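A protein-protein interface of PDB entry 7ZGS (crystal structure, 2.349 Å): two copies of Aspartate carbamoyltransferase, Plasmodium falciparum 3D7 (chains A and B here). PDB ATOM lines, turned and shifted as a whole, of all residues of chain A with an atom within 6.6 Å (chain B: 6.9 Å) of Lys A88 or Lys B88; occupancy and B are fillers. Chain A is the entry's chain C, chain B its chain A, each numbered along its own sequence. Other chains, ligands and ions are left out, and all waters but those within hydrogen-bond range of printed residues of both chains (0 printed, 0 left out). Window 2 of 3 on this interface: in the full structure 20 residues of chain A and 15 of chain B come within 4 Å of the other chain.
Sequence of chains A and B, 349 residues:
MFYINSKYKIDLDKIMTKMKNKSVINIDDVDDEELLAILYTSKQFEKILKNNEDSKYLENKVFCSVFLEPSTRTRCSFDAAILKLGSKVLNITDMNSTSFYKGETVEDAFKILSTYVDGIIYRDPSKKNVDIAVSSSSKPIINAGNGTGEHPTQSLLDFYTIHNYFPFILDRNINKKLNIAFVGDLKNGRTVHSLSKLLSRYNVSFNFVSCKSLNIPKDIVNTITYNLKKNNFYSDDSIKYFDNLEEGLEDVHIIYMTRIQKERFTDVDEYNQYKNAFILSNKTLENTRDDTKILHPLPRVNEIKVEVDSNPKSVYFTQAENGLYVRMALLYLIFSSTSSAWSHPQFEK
O of Lys B88 sits at hydrogen-bond distance from N of Phe B63, 2.9 Å away.
The backbone carbonyl oxygen of Leu A58 is in hydrogen-bond range of the side-chain hydroxyl of Ser A87 (2.5 Å).
The backbone NH (N) of Lys A61 sits close to the side-chain hydroxyl (OG) of Ser A87, 3.2 Å away.
The backbone carbonyl oxygen (O) of Lys A61 lies within hydrogen-bond range of the backbone NH (N) of Lys A88.
The backbone NH (N) of Phe A63 is in hydrogen-bond range of the backbone carbonyl oxygen (O) of Lys A88, at 2.9 Å.
O of Ile A82 sits at hydrogen-bond distance from N of Ser A87 (3.1 Å).
Of the printed residues of chain B, Leu A83 touches Val B62, Lys B88 and Val B89.
Printed residues of chain B within 4 Å of Gly A86: Lys B88 (3.8 Å).
Printed residues of chain B within 4 Å of Ser A87: Lys B88 (3.1 Å).
Printed residues of chain B within 4 Å of Lys A88: Lys B88 (3.99 Å).
Of the printed residues of chain A, Asn B60 touches Lys A56.
Printed residues of chain A within 4 Å of Val B62: Leu A83 and Lys A84.
Of the printed residues of chain A, Lys B88 touches Leu A83 (3.2 Å), Gly A86 (3.8 Å), Ser A87 (3.1 Å) and Lys A88 (3.99 Å).
Hydrophobic or aromatic side chains of chain A that line the printed part of chain B: Leu A83.
Of the 15 printed residues of chain B, 4 touch a printed residue of chain A.
Printed residues of chain B that touch a printed residue of chain A: Asn B60, Val B62, Lys B88 and Val B89.
Among the printed residues, 8 pairs touch across the chains.
Among the printed residues, no Asp or Glu carboxylate lies within 4 Å of a Lys or Arg side-chain nitrogen of the other chain.
Leu A83 touches Lys B88, but with the chains exchanged Lys A88 does not touch Leu B83 (7.1 Å).
Leu A83 touches Val B89, but with the chains exchanged Val A89 does not touch Leu B83 (9.1 Å).
Ser A87 touches Lys B88, but with the chains exchanged Lys A88 does not touch Ser B87 (7.0 Å).
Lys A88 touches its own counterpart, Lys B88.
Of the 8 pairs that touch across the chains among the printed residues, 1 has its exchanged pair printed and touching as well.
The backbone carbonyl oxygen (O) of Ser A87 lies within hydrogen-bond range of the side-chain amino group (NZ) of Lys B88, at 3.1 Å.
Lys A56 touches Asn B60 (NZ to ND2, 3.8 Å).
Leu A83 touches Val B62.
Lys B88 touches Leu A83 (CD to O, 3.2 Å).
Val B89 touches Leu A83.
Lys A84 touches Val B62.
O of Gly A86 touches NZ of Lys B88 (3.8 Å).
Lys A88 touches Lys B88.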
ATOM      1  N   LYS A  56      -5.417  13.665  14.451  1.00  0.00           N
ATOM      2  CA  LYS A  56      -4.448  14.764  14.650  1.00  0.00           C
ATOM      3  C   LYS A  56      -3.616  14.466  15.896  1.00  0.00           C
ATOM      4  O   LYS A  56      -3.778  15.167  16.890  1.00  0.00           O
ATOM      5  CB  LYS A  56      -5.191  16.096  14.705  1.00  0.00           C
ATOM      6  CG  LYS A  56      -5.819  16.556  13.394  1.00  0.00           C
ATOM      7  CD  LYS A  56      -6.387  17.977  13.452  1.00  0.00           C
ATOM      8  CE  LYS A  56      -6.575  18.559  12.070  1.00  0.00           C
ATOM      9  NZ  LYS A  56      -6.761  20.031  12.141  1.00  0.00           N
ATOM     10  N   LEU A  58      -0.217  14.481  15.945  1.00  0.00           N
ATOM     11  CA  LEU A  58       1.035  15.264  15.902  1.00  0.00           C
ATOM     12  C   LEU A  58       0.780  16.622  15.247  1.00  0.00           C
ATOM     13  O   LEU A  58       1.106  16.784  14.074  1.00  0.00           O
ATOM     14  CB  LEU A  58       2.117  14.470  15.174  1.00  0.00           C
ATOM     15  CG  LEU A  58       3.502  15.125  15.158  1.00  0.00           C
ATOM     16  CD1 LEU A  58       4.208  14.930  16.483  1.00  0.00           C
ATOM     17  CD2 LEU A  58       4.356  14.632  13.988  1.00  0.00           C
ATOM     18  N   ASN A  60       1.389  20.889  15.661  1.00  0.00           N
ATOM     19  CA  ASN A  60       2.370  21.847  16.225  1.00  0.00           C
ATOM     20  C   ASN A  60       3.742  21.647  15.577  1.00  0.00           C
ATOM     21  O   ASN A  60       4.553  22.468  15.856  1.00  0.00           O
ATOM     22  CB  ASN A  60       2.401  21.853  17.762  1.00  0.00           C
ATOM     23  CG  ASN A  60       1.028  22.070  18.365  1.00  0.00           C
ATOM     24  OD1 ASN A  60       0.636  21.338  19.265  1.00  0.00           O
ATOM     25  ND2 ASN A  60       0.270  23.033  17.853  1.00  0.00           N
ATOM     26  N   LYS A  61       3.916  20.689  14.680  1.00  0.00           N
ATOM     27  CA  LYS A  61       5.189  20.420  13.982  1.00  0.00           C
ATOM     28  C   LYS A  61       5.186  20.989  12.559  1.00  0.00           C
ATOM     29  O   LYS A  61       4.162  20.997  11.869  1.00  0.00           O
ATOM     30  CB  LYS A  61       5.521  18.922  13.948  1.00  0.00           C
ATOM     31  CG  LYS A  61       5.608  18.259  15.320  1.00  0.00           C
ATOM     32  CD  LYS A  61       6.671  18.817  16.263  1.00  0.00           C
ATOM     33  CE  LYS A  61       6.411  18.362  17.680  1.00  0.00           C
ATOM     34  NZ  LYS A  61       7.363  18.971  18.640  1.00  0.00           N
ATOM     35  N   VAL A  62       6.352  21.449  12.143  1.00  0.00           N
ATOM     36  CA  VAL A  62       6.574  22.011  10.782  1.00  0.00           C
ATOM     37  C   VAL A  62       7.723  21.217  10.172  1.00  0.00           C
ATOM     38  O   VAL A  62       8.777  21.165  10.798  1.00  0.00           O
ATOM     39  CB  VAL A  62       6.865  23.525  10.852  1.00  0.00           C
ATOM     40  CG1 VAL A  62       7.122  24.060   9.472  1.00  0.00           C
ATOM     41  CG2 VAL A  62       5.742  24.286  11.540  1.00  0.00           C
ATOM     42  N   PHE A  63       7.493  20.567   9.046  1.00  0.00           N
ATOM     43  CA  PHE A  63       8.496  19.718   8.360  1.00  0.00           C
ATOM     44  C   PHE A  63       8.910  20.434   7.094  1.00  0.00           C
ATOM     45  O   PHE A  63       8.165  21.294   6.610  1.00  0.00           O
ATOM     46  CB  PHE A  63       7.917  18.350   8.036  1.00  0.00           C
ATOM     47  CG  PHE A  63       7.570  17.522   9.240  1.00  0.00           C
ATOM     48  CD1 PHE A  63       8.524  16.690   9.810  1.00  0.00           C
ATOM     49  CD2 PHE A  63       6.322  17.573   9.815  1.00  0.00           C
ATOM     50  CE1 PHE A  63       8.235  15.936  10.947  1.00  0.00           C
ATOM     51  CE2 PHE A  63       6.029  16.811  10.935  1.00  0.00           C
ATOM     52  CZ  PHE A  63       6.978  16.000  11.502  1.00  0.00           C
ATOM     53  N   CYS A  64      10.060  20.050   6.559  1.00  0.00           N
ATOM     54  CA  CYS A  64      10.458  20.346   5.170  1.00  0.00           C
ATOM     55  C   CYS A  64      10.562  19.020   4.426  1.00  0.00           C
ATOM     56  O   CYS A  64      11.145  18.060   4.945  1.00  0.00           O
ATOM     57  CB  CYS A  64      11.731  21.161   5.054  1.00  0.00           C
ATOM     58  SG  CYS A  64      12.128  21.584   3.331  1.00  0.00           S
ATOM     59  N   ILE A  82       1.723  13.812   7.007  1.00  0.00           N
ATOM     60  CA  ILE A  82       2.047  15.012   7.834  1.00  0.00           C
ATOM     61  C   ILE A  82       0.762  15.782   8.076  1.00  0.00           C
ATOM     62  O   ILE A  82       0.457  16.125   9.261  1.00  0.00           O
ATOM     63  CB  ILE A  82       3.110  15.886   7.158  1.00  0.00           C
ATOM     64  CG1 ILE A  82       4.478  15.211   7.178  1.00  0.00           C
ATOM     65  CG2 ILE A  82       3.185  17.230   7.833  1.00  0.00           C
ATOM     66  CD1 ILE A  82       5.466  15.737   6.138  1.00  0.00           C
ATOM     67  N   LEU A  83       0.061  16.067   6.981  1.00  0.00           N
ATOM     68  CA  LEU A  83      -1.143  16.916   7.022  1.00  0.00           C
ATOM     69  C   LEU A  83      -2.234  16.201   7.847  1.00  0.00           C
ATOM     70  O   LEU A  83      -2.909  16.878   8.658  1.00  0.00           O
ATOM     71  CB  LEU A  83      -1.555  17.265   5.586  1.00  0.00           C
ATOM     72  CG  LEU A  83      -0.550  18.131   4.811  1.00  0.00           C
ATOM     73  CD1 LEU A  83      -0.997  18.312   3.372  1.00  0.00           C
ATOM     74  CD2 LEU A  83      -0.360  19.503   5.446  1.00  0.00           C
ATOM     75  N   LYS A  84      -2.380  14.888   7.706  1.00  0.00           N
ATOM     76  CA  LYS A  84      -3.471  14.145   8.389  1.00  0.00           C
ATOM     77  C   LYS A  84      -3.151  14.023   9.876  1.00  0.00           C
ATOM     78  O   LYS A  84      -4.080  13.863  10.637  1.00  0.00           O
ATOM     79  CB  LYS A  84      -3.669  12.762   7.773  1.00  0.00           C
ATOM     80  CG  LYS A  84      -4.650  12.690   6.622  1.00  0.00           C
ATOM     81  CD  LYS A  84      -6.071  13.009   7.066  1.00  0.00           C
ATOM     82  CE  LYS A  84      -6.593  11.991   8.048  1.00  0.00           C
ATOM     83  NZ  LYS A  84      -7.917  12.379   8.532  1.00  0.00           N
ATOM     84  N   LEU A  85      -1.869  14.083  10.277  1.00  0.00           N
ATOM     85  CA  LEU A  85      -1.425  14.078  11.697  1.00  0.00           C
ATOM     86  C   LEU A  85      -1.689  15.465  12.298  1.00  0.00           C
ATOM     87  O   LEU A  85      -1.666  15.582  13.561  1.00  0.00           O
ATOM     88  CB  LEU A  85       0.070  13.760  11.781  1.00  0.00           C
ATOM     89  CG  LEU A  85       0.449  12.283  11.721  1.00  0.00           C
ATOM     90  CD1 LEU A  85       1.948  12.155  11.579  1.00  0.00           C
ATOM     91  CD2 LEU A  85      -0.060  11.518  12.947  1.00  0.00           C
ATOM     92  N   GLY A  86      -1.905  16.486  11.446  1.00  0.00           N
ATOM     93  CA  GLY A  86      -2.295  17.843  11.887  1.00  0.00           C
ATOM     94  C   GLY A  86      -1.111  18.809  11.889  1.00  0.00           C
ATOM     95  O   GLY A  86      -1.274  19.973  12.262  1.00  0.00           O
ATOM     96  N   SER A  87       0.049  18.372  11.427  1.00  0.00           N
ATOM     97  CA  SER A  87       1.232  19.245  11.290  1.00  0.00           C
ATOM     98  C   SER A  87       1.226  19.927   9.925  1.00  0.00           C
ATOM     99  O   SER A  87       0.176  19.891   9.205  1.00  0.00           O
ATOM    100  CB  SER A  87       2.467  18.439  11.552  1.00  0.00           C
ATOM    101  OG  SER A  87       2.634  18.375  12.961  1.00  0.00           O
ATOM    102  N   LYS A  88       2.317  20.594   9.599  1.00  0.00           N
ATOM    103  CA  LYS A  88       2.408  21.424   8.389  1.00  0.00           C
ATOM    104  C   LYS A  88       3.719  21.107   7.682  1.00  0.00           C
ATOM    105  O   LYS A  88       4.641  20.636   8.360  1.00  0.00           O
ATOM    106  CB  LYS A  88       2.362  22.903   8.773  1.00  0.00           C
ATOM    107  CG  LYS A  88       1.004  23.440   9.226  1.00  0.00           C
ATOM    108  CD  LYS A  88       1.189  24.720  10.013  1.00  0.00           C
ATOM    109  CE  LYS A  88      -0.055  25.294  10.623  1.00  0.00           C
ATOM    110  NZ  LYS A  88      -1.071  25.497   9.560  1.00  0.00           N
ATOM    111  N   VAL A  89       3.803  21.356   6.383  1.00  0.00           N
ATOM    112  CA  VAL A  89       5.044  21.084   5.632  1.00  0.00           C
ATOM    113  C   VAL A  89       5.265  22.161   4.556  1.00  0.00           C
ATOM    114  O   VAL A  89       4.332  22.596   3.899  1.00  0.00           O
ATOM    115  CB  VAL A  89       5.020  19.636   5.060  1.00  0.00           C
ATOM    116  CG1 VAL A  89       3.826  19.369   4.173  1.00  0.00           C
ATOM    117  CG2 VAL A  89       6.316  19.288   4.318  1.00  0.00           C
ATOM    118  N   LEU A  90       6.539  22.426   4.328  1.00  0.00           N
ATOM    119  CA  LEU A  90       7.164  23.322   3.330  1.00  0.00           C
ATOM    120  C   LEU A  90       7.814  22.370   2.318  1.00  0.00           C
ATOM    121  O   LEU A  90       8.451  21.447   2.766  1.00  0.00           O
ATOM    122  CB  LEU A  90       8.066  24.144   4.269  1.00  0.00           C
ATOM    123  CG  LEU A  90       9.397  24.761   3.882  1.00  0.00           C
ATOM    124  CD1 LEU A  90      10.163  24.977   5.147  1.00  0.00           C
ATOM    125  CD2 LEU A  90      10.222  23.963   2.920  1.00  0.00           C
ATOM    126  N   LYS B  56     -13.581  28.874   9.451  1.00  0.00           N
ATOM    127  CA  LYS B  56     -13.026  27.513   9.511  1.00  0.00           C
ATOM    128  C   LYS B  56     -14.158  26.514   9.669  1.00  0.00           C
ATOM    129  O   LYS B  56     -14.219  25.887  10.716  1.00  0.00           O
ATOM    130  CB  LYS B  56     -11.984  27.388  10.629  1.00  0.00           C
ATOM    131  CG  LYS B  56     -10.673  28.113  10.378  1.00  0.00           C
ATOM    132  CD  LYS B  56      -9.747  28.008  11.583  1.00  0.00           C
ATOM    133  CE  LYS B  56      -8.301  28.355  11.266  1.00  0.00           C
ATOM    134  NZ  LYS B  56      -7.568  27.243  10.615  1.00  0.00           N
ATOM    135  N   LEU B  58     -14.651  23.839   7.709  1.00  0.00           N
ATOM    136  CA  LEU B  58     -14.230  22.515   7.196  1.00  0.00           C
ATOM    137  C   LEU B  58     -12.756  22.336   7.499  1.00  0.00           C
ATOM    138  O   LEU B  58     -11.946  22.484   6.608  1.00  0.00           O
ATOM    139  CB  LEU B  58     -14.490  22.375   5.692  1.00  0.00           C
ATOM    140  CG  LEU B  58     -14.287  20.964   5.142  1.00  0.00           C
ATOM    141  CD1 LEU B  58     -15.522  20.121   5.454  1.00  0.00           C
ATOM    142  CD2 LEU B  58     -14.017  20.969   3.642  1.00  0.00           C
ATOM    143  N   GLU B  59     -12.439  22.096   8.754  1.00  0.00           N
ATOM    144  CA  GLU B  59     -11.086  21.716   9.197  1.00  0.00           C
ATOM    145  C   GLU B  59     -11.105  20.196   9.207  1.00  0.00           C
ATOM    146  O   GLU B  59     -12.198  19.620   9.029  1.00  0.00           O
ATOM    147  CB  GLU B  59     -10.783  22.352  10.551  1.00  0.00           C
ATOM    148  CG  GLU B  59     -11.944  22.307  11.528  1.00  0.00           C
ATOM    149  CD  GLU B  59     -12.111  23.567  12.357  1.00  0.00           C
ATOM    150  OE1 GLU B  59     -13.219  23.776  12.905  1.00  0.00           O
ATOM    151  OE2 GLU B  59     -11.121  24.316  12.474  1.00  0.00           O
ATOM    152  N   ASN B  60      -9.956  19.565   9.385  1.00  0.00           N
ATOM    153  CA  ASN B  60      -9.848  18.089   9.590  1.00  0.00           C
ATOM    154  C   ASN B  60      -9.843  17.371   8.243  1.00  0.00           C
ATOM    155  O   ASN B  60      -9.649  16.180   8.286  1.00  0.00           O
ATOM    156  CB  ASN B  60     -10.873  17.497  10.584  1.00  0.00           C
ATOM    157  CG  ASN B  60     -10.440  17.603  12.045  1.00  0.00           C
ATOM    158  OD1 ASN B  60     -10.220  16.579  12.715  1.00  0.00           O
ATOM    159  ND2 ASN B  60     -10.288  18.825  12.558  1.00  0.00           N
ATOM    160  N   LYS B  61      -9.955  18.085   7.115  1.00  0.00           N
ATOM    161  CA  LYS B  61      -9.812  17.500   5.768  1.00  0.00           C
ATOM    162  C   LYS B  61      -8.429  17.782   5.161  1.00  0.00           C
ATOM    163  O   LYS B  61      -7.842  18.846   5.354  1.00  0.00           O
ATOM    164  CB  LYS B  61     -10.911  17.973   4.828  1.00  0.00           C
ATOM    165  CG  LYS B  61     -12.323  17.673   5.325  1.00  0.00           C
ATOM    166  CD  LYS B  61     -12.705  16.214   5.258  1.00  0.00           C
ATOM    167  CE  LYS B  61     -13.813  15.849   6.225  1.00  0.00           C
ATOM    168  NZ  LYS B  61     -14.050  14.390   6.229  1.00  0.00           N
ATOM    169  N   VAL B  62      -7.952  16.825   4.389  1.00  0.00           N
ATOM    170  CA  VAL B  62      -6.711  16.947   3.597  1.00  0.00           C
ATOM    171  C   VAL B  62      -7.083  16.649   2.141  1.00  0.00           C
ATOM    172  O   VAL B  62      -7.625  15.585   1.883  1.00  0.00           O
ATOM    173  CB  VAL B  62      -5.658  15.960   4.130  1.00  0.00           C
ATOM    174  CG1 VAL B  62      -4.413  15.968   3.278  1.00  0.00           C
ATOM    175  CG2 VAL B  62      -5.351  16.183   5.593  1.00  0.00           C
ATOM    176  N   PHE B  63      -6.824  17.568   1.240  1.00  0.00           N
ATOM    177  CA  PHE B  63      -7.127  17.444  -0.198  1.00  0.00           C
ATOM    178  C   PHE B  63      -5.802  17.284  -0.933  1.00  0.00           C
ATOM    179  O   PHE B  63      -4.746  17.638  -0.400  1.00  0.00           O
ATOM    180  CB  PHE B  63      -7.869  18.691  -0.706  1.00  0.00           C
ATOM    181  CG  PHE B  63      -9.222  18.870  -0.081  1.00  0.00           C
ATOM    182  CD1 PHE B  63     -10.343  18.239  -0.601  1.00  0.00           C
ATOM    183  CD2 PHE B  63      -9.380  19.660   1.052  1.00  0.00           C
ATOM    184  CE1 PHE B  63     -11.588  18.412  -0.018  1.00  0.00           C
ATOM    185  CE2 PHE B  63     -10.633  19.812   1.631  1.00  0.00           C
ATOM    186  CZ  PHE B  63     -11.732  19.205   1.086  1.00  0.00           C
ATOM    187  N   CYS B  64      -5.895  16.798  -2.159  1.00  0.00           N
ATOM    188  CA  CYS B  64      -4.807  16.890  -3.146  1.00  0.00           C
ATOM    189  C   CYS B  64      -5.327  17.728  -4.310  1.00  0.00           C
ATOM    190  O   CYS B  64      -6.449  17.490  -4.801  1.00  0.00           O
ATOM    191  CB  CYS B  64      -4.338  15.518  -3.618  1.00  0.00           C
ATOM    192  SG  CYS B  64      -3.030  15.652  -4.849  1.00  0.00           S
ATOM    193  N   ILE B  82      -9.714  26.168   0.308  1.00  0.00           N
ATOM    194  CA  ILE B  82      -9.453  24.993   1.176  1.00  0.00           C
ATOM    195  C   ILE B  82      -8.824  25.516   2.456  1.00  0.00           C
ATOM    196  O   ILE B  82      -9.236  25.141   3.561  1.00  0.00           O
ATOM    197  CB  ILE B  82      -8.525  23.983   0.466  1.00  0.00           C
ATOM    198  CG1 ILE B  82      -9.204  23.300  -0.718  1.00  0.00           C
ATOM    199  CG2 ILE B  82      -7.976  22.977   1.453  1.00  0.00           C
ATOM    200  CD1 ILE B  82      -8.211  22.684  -1.733  1.00  0.00           C
ATOM    201  N   LEU B  83      -7.794  26.334   2.295  1.00  0.00           N
ATOM    202  CA  LEU B  83      -7.012  26.835   3.448  1.00  0.00           C
ATOM    203  C   LEU B  83      -7.891  27.750   4.310  1.00  0.00           C
ATOM    204  O   LEU B  83      -7.818  27.651   5.516  1.00  0.00           O
ATOM    205  CB  LEU B  83      -5.732  27.492   2.942  1.00  0.00           C
ATOM    206  CG  LEU B  83      -4.760  26.540   2.238  1.00  0.00           C
ATOM    207  CD1 LEU B  83      -3.614  27.323   1.589  1.00  0.00           C
ATOM    208  CD2 LEU B  83      -4.226  25.523   3.211  1.00  0.00           C
ATOM    209  N   GLY B  86     -10.017  25.998   6.615  1.00  0.00           N
ATOM    210  CA  GLY B  86      -9.211  25.462   7.725  1.00  0.00           C
ATOM    211  C   GLY B  86      -8.667  24.078   7.399  1.00  0.00           C
ATOM    212  O   GLY B  86      -8.038  23.490   8.238  1.00  0.00           O
ATOM    213  N   SER B  87      -8.854  23.596   6.188  1.00  0.00           N
ATOM    214  CA  SER B  87      -8.326  22.266   5.794  1.00  0.00           C
ATOM    215  C   SER B  87      -6.915  22.421   5.226  1.00  0.00           C
ATOM    216  O   SER B  87      -6.278  23.503   5.392  1.00  0.00           O
ATOM    217  CB  SER B  87      -9.290  21.554   4.888  1.00  0.00           C
ATOM    218  OG  SER B  87     -10.260  20.913   5.720  1.00  0.00           O
ATOM    219  N   LYS B  88      -6.392  21.347   4.691  1.00  0.00           N
ATOM    220  CA  LYS B  88      -4.999  21.306   4.222  1.00  0.00           C
ATOM    221  C   LYS B  88      -5.002  20.754   2.812  1.00  0.00           C
ATOM    222  O   LYS B  88      -5.910  20.034   2.480  1.00  0.00           O
ATOM    223  CB  LYS B  88      -4.145  20.414   5.114  1.00  0.00           C
ATOM    224  CG  LYS B  88      -3.889  20.920   6.525  1.00  0.00           C
ATOM    225  CD  LYS B  88      -3.293  19.843   7.397  1.00  0.00           C
ATOM    226  CE  LYS B  88      -3.269  20.276   8.829  1.00  0.00           C
ATOM    227  NZ  LYS B  88      -2.466  21.497   8.969  1.00  0.00           N
ATOM    228  N   VAL B  89      -3.986  21.090   2.057  1.00  0.00           N
ATOM    229  CA  VAL B  89      -3.855  20.577   0.678  1.00  0.00           C
ATOM    230  C   VAL B  89      -2.362  20.324   0.376  1.00  0.00           C
ATOM    231  O   VAL B  89      -1.479  21.098   0.764  1.00  0.00           O
ATOM    232  CB  VAL B  89      -4.566  21.486  -0.343  1.00  0.00           C
ATOM    233  CG1 VAL B  89      -4.089  22.906  -0.298  1.00  0.00           C
ATOM    234  CG2 VAL B  89      -4.449  20.958  -1.747  1.00  0.00           C
ATOM    235  N   LEU B  90      -2.176  19.262  -0.377  1.00  0.00           N
ATOM    236  CA  LEU B  90      -0.948  18.720  -0.956  1.00  0.00           C
ATOM    237  C   LEU B  90      -1.073  19.037  -2.454  1.00  0.00           C
ATOM    238  O   LEU B  90      -2.168  18.837  -3.003  1.00  0.00           O
ATOM    239  CB  LEU B  90      -1.105  17.256  -0.491  1.00  0.00           C
ATOM    240  CG  LEU B  90      -0.611  16.051  -1.267  1.00  0.00           C
ATOM    241  CD1 LEU B  90      -1.416  14.875  -0.814  1.00  0.00           C
ATOM    242  CD2 LEU B  90      -0.703  16.159  -2.767  1.00  0.00           C
